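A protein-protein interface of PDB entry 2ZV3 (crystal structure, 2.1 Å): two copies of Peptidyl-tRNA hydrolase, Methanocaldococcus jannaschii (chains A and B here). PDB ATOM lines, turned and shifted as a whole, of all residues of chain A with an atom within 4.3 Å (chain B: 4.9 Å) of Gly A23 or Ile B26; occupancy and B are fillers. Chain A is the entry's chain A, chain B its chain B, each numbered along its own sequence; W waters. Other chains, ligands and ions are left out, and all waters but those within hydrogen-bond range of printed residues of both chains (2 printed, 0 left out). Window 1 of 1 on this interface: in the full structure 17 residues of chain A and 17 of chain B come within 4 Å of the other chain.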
ATOM      1  N   VAL A  19      24.401  -2.399  21.665  1.00  0.00           N
ATOM      2  CA  VAL A  19      24.502  -1.883  23.029  1.00  0.00           C
ATOM      3  C   VAL A  19      25.289  -0.575  23.031  1.00  0.00           C
ATOM      4  O   VAL A  19      24.899   0.390  23.686  1.00  0.00           O
ATOM      5  CB  VAL A  19      25.175  -2.905  23.975  1.00  0.00           C
ATOM      6  CG1 VAL A  19      25.200  -2.362  25.400  1.00  0.00           C
ATOM      7  CG2 VAL A  19      24.418  -4.209  23.940  1.00  0.00           C
ATOM      8  N   ALA A  20      26.382  -0.536  22.275  1.00  0.00           N
ATOM      9  CA  ALA A  20      27.209   0.670  22.179  1.00  0.00           C
ATOM     10  C   ALA A  20      26.467   1.818  21.506  1.00  0.00           C
ATOM     11  O   ALA A  20      26.463   2.940  22.007  1.00  0.00           O
ATOM     12  CB  ALA A  20      28.499   0.370  21.398  1.00  0.00           C
ATOM     13  N   GLN A  21      25.842   1.531  20.366  1.00  0.00           N
ATOM     14  CA  GLN A  21      25.146   2.560  19.607  1.00  0.00           C
ATOM     15  C   GLN A  21      23.921   3.078  20.374  1.00  0.00           C
ATOM     16  O   GLN A  21      23.675   4.270  20.482  1.00  0.00           O
ATOM     17  CB  GLN A  21      24.729   1.985  18.252  1.00  0.00           C
ATOM     18  CG  GLN A  21      25.919   1.629  17.364  1.00  0.00           C
ATOM     19  CD  GLN A  21      26.754   2.859  17.091  1.00  0.00           C
ATOM     20  OE1 GLN A  21      26.295   3.898  16.636  1.00  0.00           O
ATOM     21  NE2 GLN A  21      28.068   2.679  17.344  1.00  0.00           N
ATOM     22  N   GLY A  22      23.112   2.137  20.895  1.00  0.00           N
ATOM     23  CA  GLY A  22      22.018   2.571  21.751  1.00  0.00           C
ATOM     24  C   GLY A  22      22.578   3.369  22.924  1.00  0.00           C
ATOM     25  O   GLY A  22      21.999   4.335  23.424  1.00  0.00           O
ATOM     26  N   GLY A  23      23.752   2.894  23.382  1.00  0.00           N
ATOM     27  CA  GLY A  23      24.432   3.532  24.492  1.00  0.00           C
ATOM     28  C   GLY A  23      24.718   5.008  24.217  1.00  0.00           C
ATOM     29  O   GLY A  23      24.503   5.869  25.060  1.00  0.00           O
ATOM     30  N   HIS A  24      25.214   5.321  23.023  1.00  0.00           N
ATOM     31  CA  HIS A  24      25.480   6.711  22.645  1.00  0.00           C
ATOM     32  C   HIS A  24      24.144   7.457  22.625  1.00  0.00           C
ATOM     33  O   HIS A  24      24.051   8.603  23.055  1.00  0.00           O
ATOM     34  CB  HIS A  24      26.086   6.805  21.232  1.00  0.00           C
ATOM     35  CG  HIS A  24      27.351   6.031  21.049  1.00  0.00           C
ATOM     36  ND1 HIS A  24      28.313   5.929  22.029  1.00  0.00           N
ATOM     37  CD2 HIS A  24      27.843   5.374  19.968  1.00  0.00           C
ATOM     38  CE1 HIS A  24      29.344   5.244  21.562  1.00  0.00           C
ATOM     39  NE2 HIS A  24      29.082   4.896  20.315  1.00  0.00           N
ATOM     40  N   ALA A  25      23.112   6.796  22.107  1.00  0.00           N
ATOM     41  CA  ALA A  25      21.775   7.399  22.012  1.00  0.00           C
ATOM     42  C   ALA A  25      21.239   7.756  23.402  1.00  0.00           C
ATOM     43  O   ALA A  25      20.726   8.850  23.629  1.00  0.00           O
ATOM     44  CB  ALA A  25      20.815   6.426  21.318  1.00  0.00           C
ATOM     45  N   ILE A  26      21.371   6.822  24.328  1.00  0.00           N
ATOM     46  CA  ILE A  26      20.891   7.018  25.694  1.00  0.00           C
ATOM     47  C   ILE A  26      21.571   8.210  26.364  1.00  0.00           C
ATOM     48  O   ILE A  26      20.905   9.089  26.896  1.00  0.00           O
ATOM     49  CB  ILE A  26      21.119   5.740  26.524  1.00  0.00           C
ATOM     50  CG1 ILE A  26      20.184   4.632  26.011  1.00  0.00           C
ATOM     51  CG2 ILE A  26      20.877   6.019  28.017  1.00  0.00           C
ATOM     52  CD1 ILE A  26      20.637   3.215  26.382  1.00  0.00           C
ATOM     53  N   ILE A  27      22.898   8.242  26.320  1.00  0.00           N
ATOM     54  CA  ILE A  27      23.655   9.337  26.921  1.00  0.00           C
ATOM     55  C   ILE A  27      23.260  10.694  26.335  1.00  0.00           C
ATOM     56  O   ILE A  27      23.057  11.666  27.067  1.00  0.00           O
ATOM     57  CB  ILE A  27      25.187   9.132  26.712  1.00  0.00           C
ATOM     58  CG1 ILE A  27      25.696   8.033  27.644  1.00  0.00           C
ATOM     59  CG2 ILE A  27      25.921  10.429  26.926  1.00  0.00           C
ATOM     60  CD1 ILE A  27      25.629   8.389  29.121  1.00  0.00           C
ATOM     61  N   MET B   3      34.636   4.046  27.713  1.00  0.00           N
ATOM     62  CA  MET B   3      33.866   3.391  28.747  1.00  0.00           C
ATOM     63  C   MET B   3      33.723   1.955  28.315  1.00  0.00           C
ATOM     64  O   MET B   3      33.490   1.671  27.139  1.00  0.00           O
ATOM     65  CB  MET B   3      32.475   4.026  28.881  1.00  0.00           C
ATOM     66  CG  MET B   3      31.539   3.288  29.848  1.00  0.00           C
ATOM     67  SD  MET B   3      29.831   3.913  29.816  1.00  0.00           S
ATOM     68  CE  MET B   3      30.042   5.552  30.507  1.00  0.00           C
ATOM     69  N   VAL B   5      31.600  -1.478  28.746  1.00  0.00           N
ATOM     70  CA  VAL B   5      30.329  -1.988  29.245  1.00  0.00           C
ATOM     71  C   VAL B   5      30.442  -3.510  29.289  1.00  0.00           C
ATOM     72  O   VAL B   5      30.773  -4.147  28.288  1.00  0.00           O
ATOM     73  CB  VAL B   5      29.147  -1.574  28.325  1.00  0.00           C
ATOM     74  CG1 VAL B   5      27.817  -2.031  28.941  1.00  0.00           C
ATOM     75  CG2 VAL B   5      29.139  -0.059  28.138  1.00  0.00           C
ATOM     76  N   GLY B  22      22.512  -2.626  29.640  1.00  0.00           N
ATOM     77  CA  GLY B  22      23.743  -1.901  29.382  1.00  0.00           C
ATOM     78  C   GLY B  22      23.505  -0.402  29.545  1.00  0.00           C
ATOM     79  O   GLY B  22      24.349   0.364  30.004  1.00  0.00           O
ATOM     80  N   GLY B  23      22.298   0.007  29.112  1.00  0.00           N
ATOM     81  CA  GLY B  23      21.916   1.404  29.206  1.00  0.00           C
ATOM     82  C   GLY B  23      21.880   1.891  30.656  1.00  0.00           C
ATOM     83  O   GLY B  23      22.355   2.969  30.981  1.00  0.00           O
ATOM     84  N   HIS B  24      21.284   1.107  31.553  1.00  0.00           N
ATOM     85  CA  HIS B  24      21.234   1.529  32.953  1.00  0.00           C
ATOM     86  C   HIS B  24      22.681   1.626  33.481  1.00  0.00           C
ATOM     87  O   HIS B  24      23.035   2.573  34.181  1.00  0.00           O
ATOM     88  CB  HIS B  24      20.440   0.529  33.819  1.00  0.00           C
ATOM     89  CG  HIS B  24      19.044   0.265  33.334  1.00  0.00           C
ATOM     90  ND1 HIS B  24      18.229   1.251  32.821  1.00  0.00           N
ATOM     91  CD2 HIS B  24      18.306  -0.873  33.326  1.00  0.00           C
ATOM     92  CE1 HIS B  24      17.051   0.736  32.518  1.00  0.00           C
ATOM     93  NE2 HIS B  24      17.071  -0.552  32.816  1.00  0.00           N
ATOM     94  N   ALA B  25      23.513   0.652  33.122  1.00  0.00           N
ATOM     95  CA  ALA B  25      24.908   0.642  33.568  1.00  0.00           C
ATOM     96  C   ALA B  25      25.631   1.890  33.075  1.00  0.00           C
ATOM     97  O   ALA B  25      26.297   2.572  33.846  1.00  0.00           O
ATOM     98  CB  ALA B  25      25.620  -0.612  33.050  1.00  0.00           C
ATOM     99  N   ILE B  26      25.488   2.180  31.783  1.00  0.00           N
ATOM    100  CA  ILE B  26      26.123   3.345  31.156  1.00  0.00           C
ATOM    101  C   ILE B  26      25.734   4.646  31.853  1.00  0.00           C
ATOM    102  O   ILE B  26      26.584   5.500  32.145  1.00  0.00           O
ATOM    103  CB  ILE B  26      25.750   3.418  29.656  1.00  0.00           C
ATOM    104  CG1 ILE B  26      26.432   2.261  28.915  1.00  0.00           C
ATOM    105  CG2 ILE B  26      26.172   4.755  29.052  1.00  0.00           C
ATOM    106  CD1 ILE B  26      25.880   1.987  27.525  1.00  0.00           C
ATOM    107  N   ILE B  27      24.445   4.808  32.110  1.00  0.00           N
ATOM    108  CA  ILE B  27      23.978   6.007  32.788  1.00  0.00           C
ATOM    109  C   ILE B  27      24.594   6.080  34.194  1.00  0.00           C
ATOM    110  O   ILE B  27      25.088   7.123  34.601  1.00  0.00           O
ATOM    111  CB  ILE B  27      22.429   6.009  32.936  1.00  0.00           C
ATOM    112  CG1 ILE B  27      21.762   6.350  31.595  1.00  0.00           C
ATOM    113  CG2 ILE B  27      22.012   6.980  34.038  1.00  0.00           C
ATOM    114  CD1 ILE B  27      22.028   7.757  31.099  1.00  0.00           C
ATOM    115  N   GLU B  28      24.564   4.967  34.926  1.00  0.00           N
ATOM    116  CA  GLU B  28      25.082   4.954  36.295  1.00  0.00           C
ATOM    117  C   GLU B  28      26.579   5.216  36.403  1.00  0.00           C
ATOM    118  O   GLU B  28      27.011   5.938  37.298  1.00  0.00           O
ATOM    119  CB  GLU B  28      24.728   3.637  37.002  1.00  0.00           C
ATOM    120  CG  GLU B  28      23.246   3.502  37.397  1.00  0.00           C
ATOM    121  CD  GLU B  28      22.756   4.643  38.280  1.00  0.00           C
ATOM    122  OE1 GLU B  28      22.964   4.575  39.506  1.00  0.00           O
ATOM    123  OE2 GLU B  28      22.176   5.612  37.755  1.00  0.00           O
ATOM    124  N   ALA B  29      27.369   4.639  35.500  1.00  0.00           N
ATOM    125  CA  ALA B  29      28.811   4.857  35.526  1.00  0.00           C
ATOM    126  C   ALA B  29      29.102   6.300  35.149  1.00  0.00           C
ATOM    127  O   ALA B  29      29.999   6.930  35.715  1.00  0.00           O
ATOM    128  CB  ALA B  29      29.501   3.921  34.572  1.00  0.00           C
ATOM    129  N   PHE B  30      28.325   6.830  34.205  1.00  0.00           N
ATOM    130  CA  PHE B  30      28.477   8.210  33.749  1.00  0.00           C
ATOM    131  C   PHE B  30      28.281   9.183  34.908  1.00  0.00           C
ATOM    132  O   PHE B  30      29.081  10.098  35.107  1.00  0.00           O
ATOM    133  CB  PHE B  30      27.446   8.520  32.662  1.00  0.00           C
ATOM    134  CG  PHE B  30      27.447   9.952  32.208  1.00  0.00           C
ATOM    135  CD1 PHE B  30      28.374  10.402  31.282  1.00  0.00           C
ATOM    136  CD2 PHE B  30      26.522  10.850  32.712  1.00  0.00           C
ATOM    137  CE1 PHE B  30      28.377  11.735  30.865  1.00  0.00           C
ATOM    138  CE2 PHE B  30      26.519  12.184  32.304  1.00  0.00           C
ATOM    139  CZ  PHE B  30      27.452  12.625  31.373  1.00  0.00           C
ATOM    140  N   GLN B  49      32.492   9.868  22.871  1.00  0.00           N
ATOM    141  CA  GLN B  49      32.143   8.956  23.954  1.00  0.00           C
ATOM    142  C   GLN B  49      32.263   7.481  23.614  1.00  0.00           C
ATOM    143  O   GLN B  49      31.318   6.706  23.768  1.00  0.00           O
ATOM    144  CB  GLN B  49      30.722   9.269  24.451  1.00  0.00           C
ATOM    145  CG  GLN B  49      29.682   9.448  23.351  1.00  0.00           C
ATOM    146  CD  GLN B  49      28.279   9.683  23.904  1.00  0.00           C
ATOM    147  OE1 GLN B  49      27.707   8.814  24.550  1.00  0.00           O
ATOM    148  NE2 GLN B  49      27.733  10.868  23.659  1.00  0.00           N
ATOM    149  N   LYS B  51      32.634   3.635  23.442  1.00  0.00           N
ATOM    150  CA  LYS B  51      32.204   2.591  24.357  1.00  0.00           C
ATOM    151  C   LYS B  51      32.564   1.251  23.747  1.00  0.00           C
ATOM    152  O   LYS B  51      32.350   1.032  22.557  1.00  0.00           O
ATOM    153  CB  LYS B  51      30.690   2.639  24.565  1.00  0.00           C
ATOM    154  CG  LYS B  51      30.186   3.913  25.180  1.00  0.00           C
ATOM    155  CD  LYS B  51      28.671   3.989  25.113  1.00  0.00           C
ATOM    156  CE  LYS B  51      28.178   5.334  25.617  1.00  0.00           C
ATOM    157  NZ  LYS B  51      28.613   6.434  24.746  1.00  0.00           N
ATOM    158  N   SER B  77      29.767   1.079  37.788  1.00  0.00           N
ATOM    159  CA  SER B  77      28.433   0.743  38.243  1.00  0.00           C
ATOM    160  C   SER B  77      28.153  -0.726  38.039  1.00  0.00           C
ATOM    161  O   SER B  77      28.824  -1.405  37.257  1.00  0.00           O
ATOM    162  CB  SER B  77      27.389   1.560  37.473  1.00  0.00           C
ATOM    163  OG  SER B  77      27.302   1.129  36.117  1.00  0.00           O
ATOM    164  N   ALA B  96      29.380  -1.189  34.147  1.00  0.00           N
ATOM    165  CA  ALA B  96      29.974  -0.199  33.253  1.00  0.00           C
ATOM    166  C   ALA B  96      31.102   0.423  34.037  1.00  0.00           C
ATOM    167  O   ALA B  96      30.931   0.783  35.201  1.00  0.00           O
ATOM    168  CB  ALA B  96      28.967   0.880  32.846  1.00  0.00           C
HETATM  169  O   HOH W   1      23.072   0.436  25.924  1.00  0.00           O
HETATM  170  O   HOH W   2      31.978   3.544  20.458  1.00  0.00           O
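A ring nitrogen (ND1) of His A24 sits at hydrogen-bond distance from the side-chain amino group (NZ) of Lys B51, at 2.8 Å.
The side-chain amide oxygen (OE1) of Gln B49 is in hydrogen-bond range of the side-chain amino group (NZ) of Lys B51, at 2.6 Å.
O of Ala A20 touches CD of Lys B51, at 3.95 Å. Ile B26 touches Gly A23 (CD1 to CA, 3.7 Å). Gly A23 touches Lys B51 (C to CE, 3.7 Å). His A24 touches Gln B49 (CE1 to O, 3.3 Å). CA of Gly B23 touches CD1 of Ile A26, 3.6 Å away. Ile B27 touches Ile A26. Ile B26 touches Ile A27 (CG2 to CG1, 3.6 Å). CD1 of Ile A27 touches CG of Phe B30 (3.9 Å). Ile A27 touches Gln B49.
Of chain B, only Ile B26 (3.7 Å) and Lys B51 (3.7 Å) come within 4 Å of Gly A23. Printed residues of chain B within 4 Å of Ile A27: Ile B26, Phe B30 and Gln B49. Of the printed residues of chain A, Gly B23 touches Ile A26 (3.6 Å). Ile B26 touches two residues of chain A. Of the printed residues of chain A, Ile B27 touches Ile A26 (3.7 Å). Of the printed residues of chain A, Phe B30 touches Ile A27 (3.9 Å). Of the printed residues of chain A, Gln B49 touches His A24 (3.3 Å) and Ile A27 (3.3 Å). The nearest residue of chain B that does not touch Gly A23 is Gln B49 (4.4 Å). The nearest printed residue of chain A that does not touch Ile B26 is Val A19 (4.3 Å).
Hydrophobic or aromatic side chains of chain B that line the printed part of chain A: Ile B26, Ile B27 and Phe B30. Along chain B the printed residues that touch a printed residue of chain A span positions 23 to 51. Among the printed residues, 10 pairs touch across the chains. Among the printed residues, no Asp or Glu carboxylate lies within 4 Å of a Lys or Arg side-chain nitrogen of the other chain.
Gly A23 touches Ile B26, and with the chains exchanged Ile A26 touches Gly B23. Ile A26 touches Ile B27, and with the chains exchanged Ile A27 touches Ile B26. Of the 10 pairs that touch across the chains among the printed residues, 4 have their exchanged pair printed and touching as well.
Water W1 bridges O of Val A19 and N of Gly B23. Water W2 lies within hydrogen-bond range of N of Lys B51 (3.1 Å) and NE2 of His A24 (3.2 Å).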
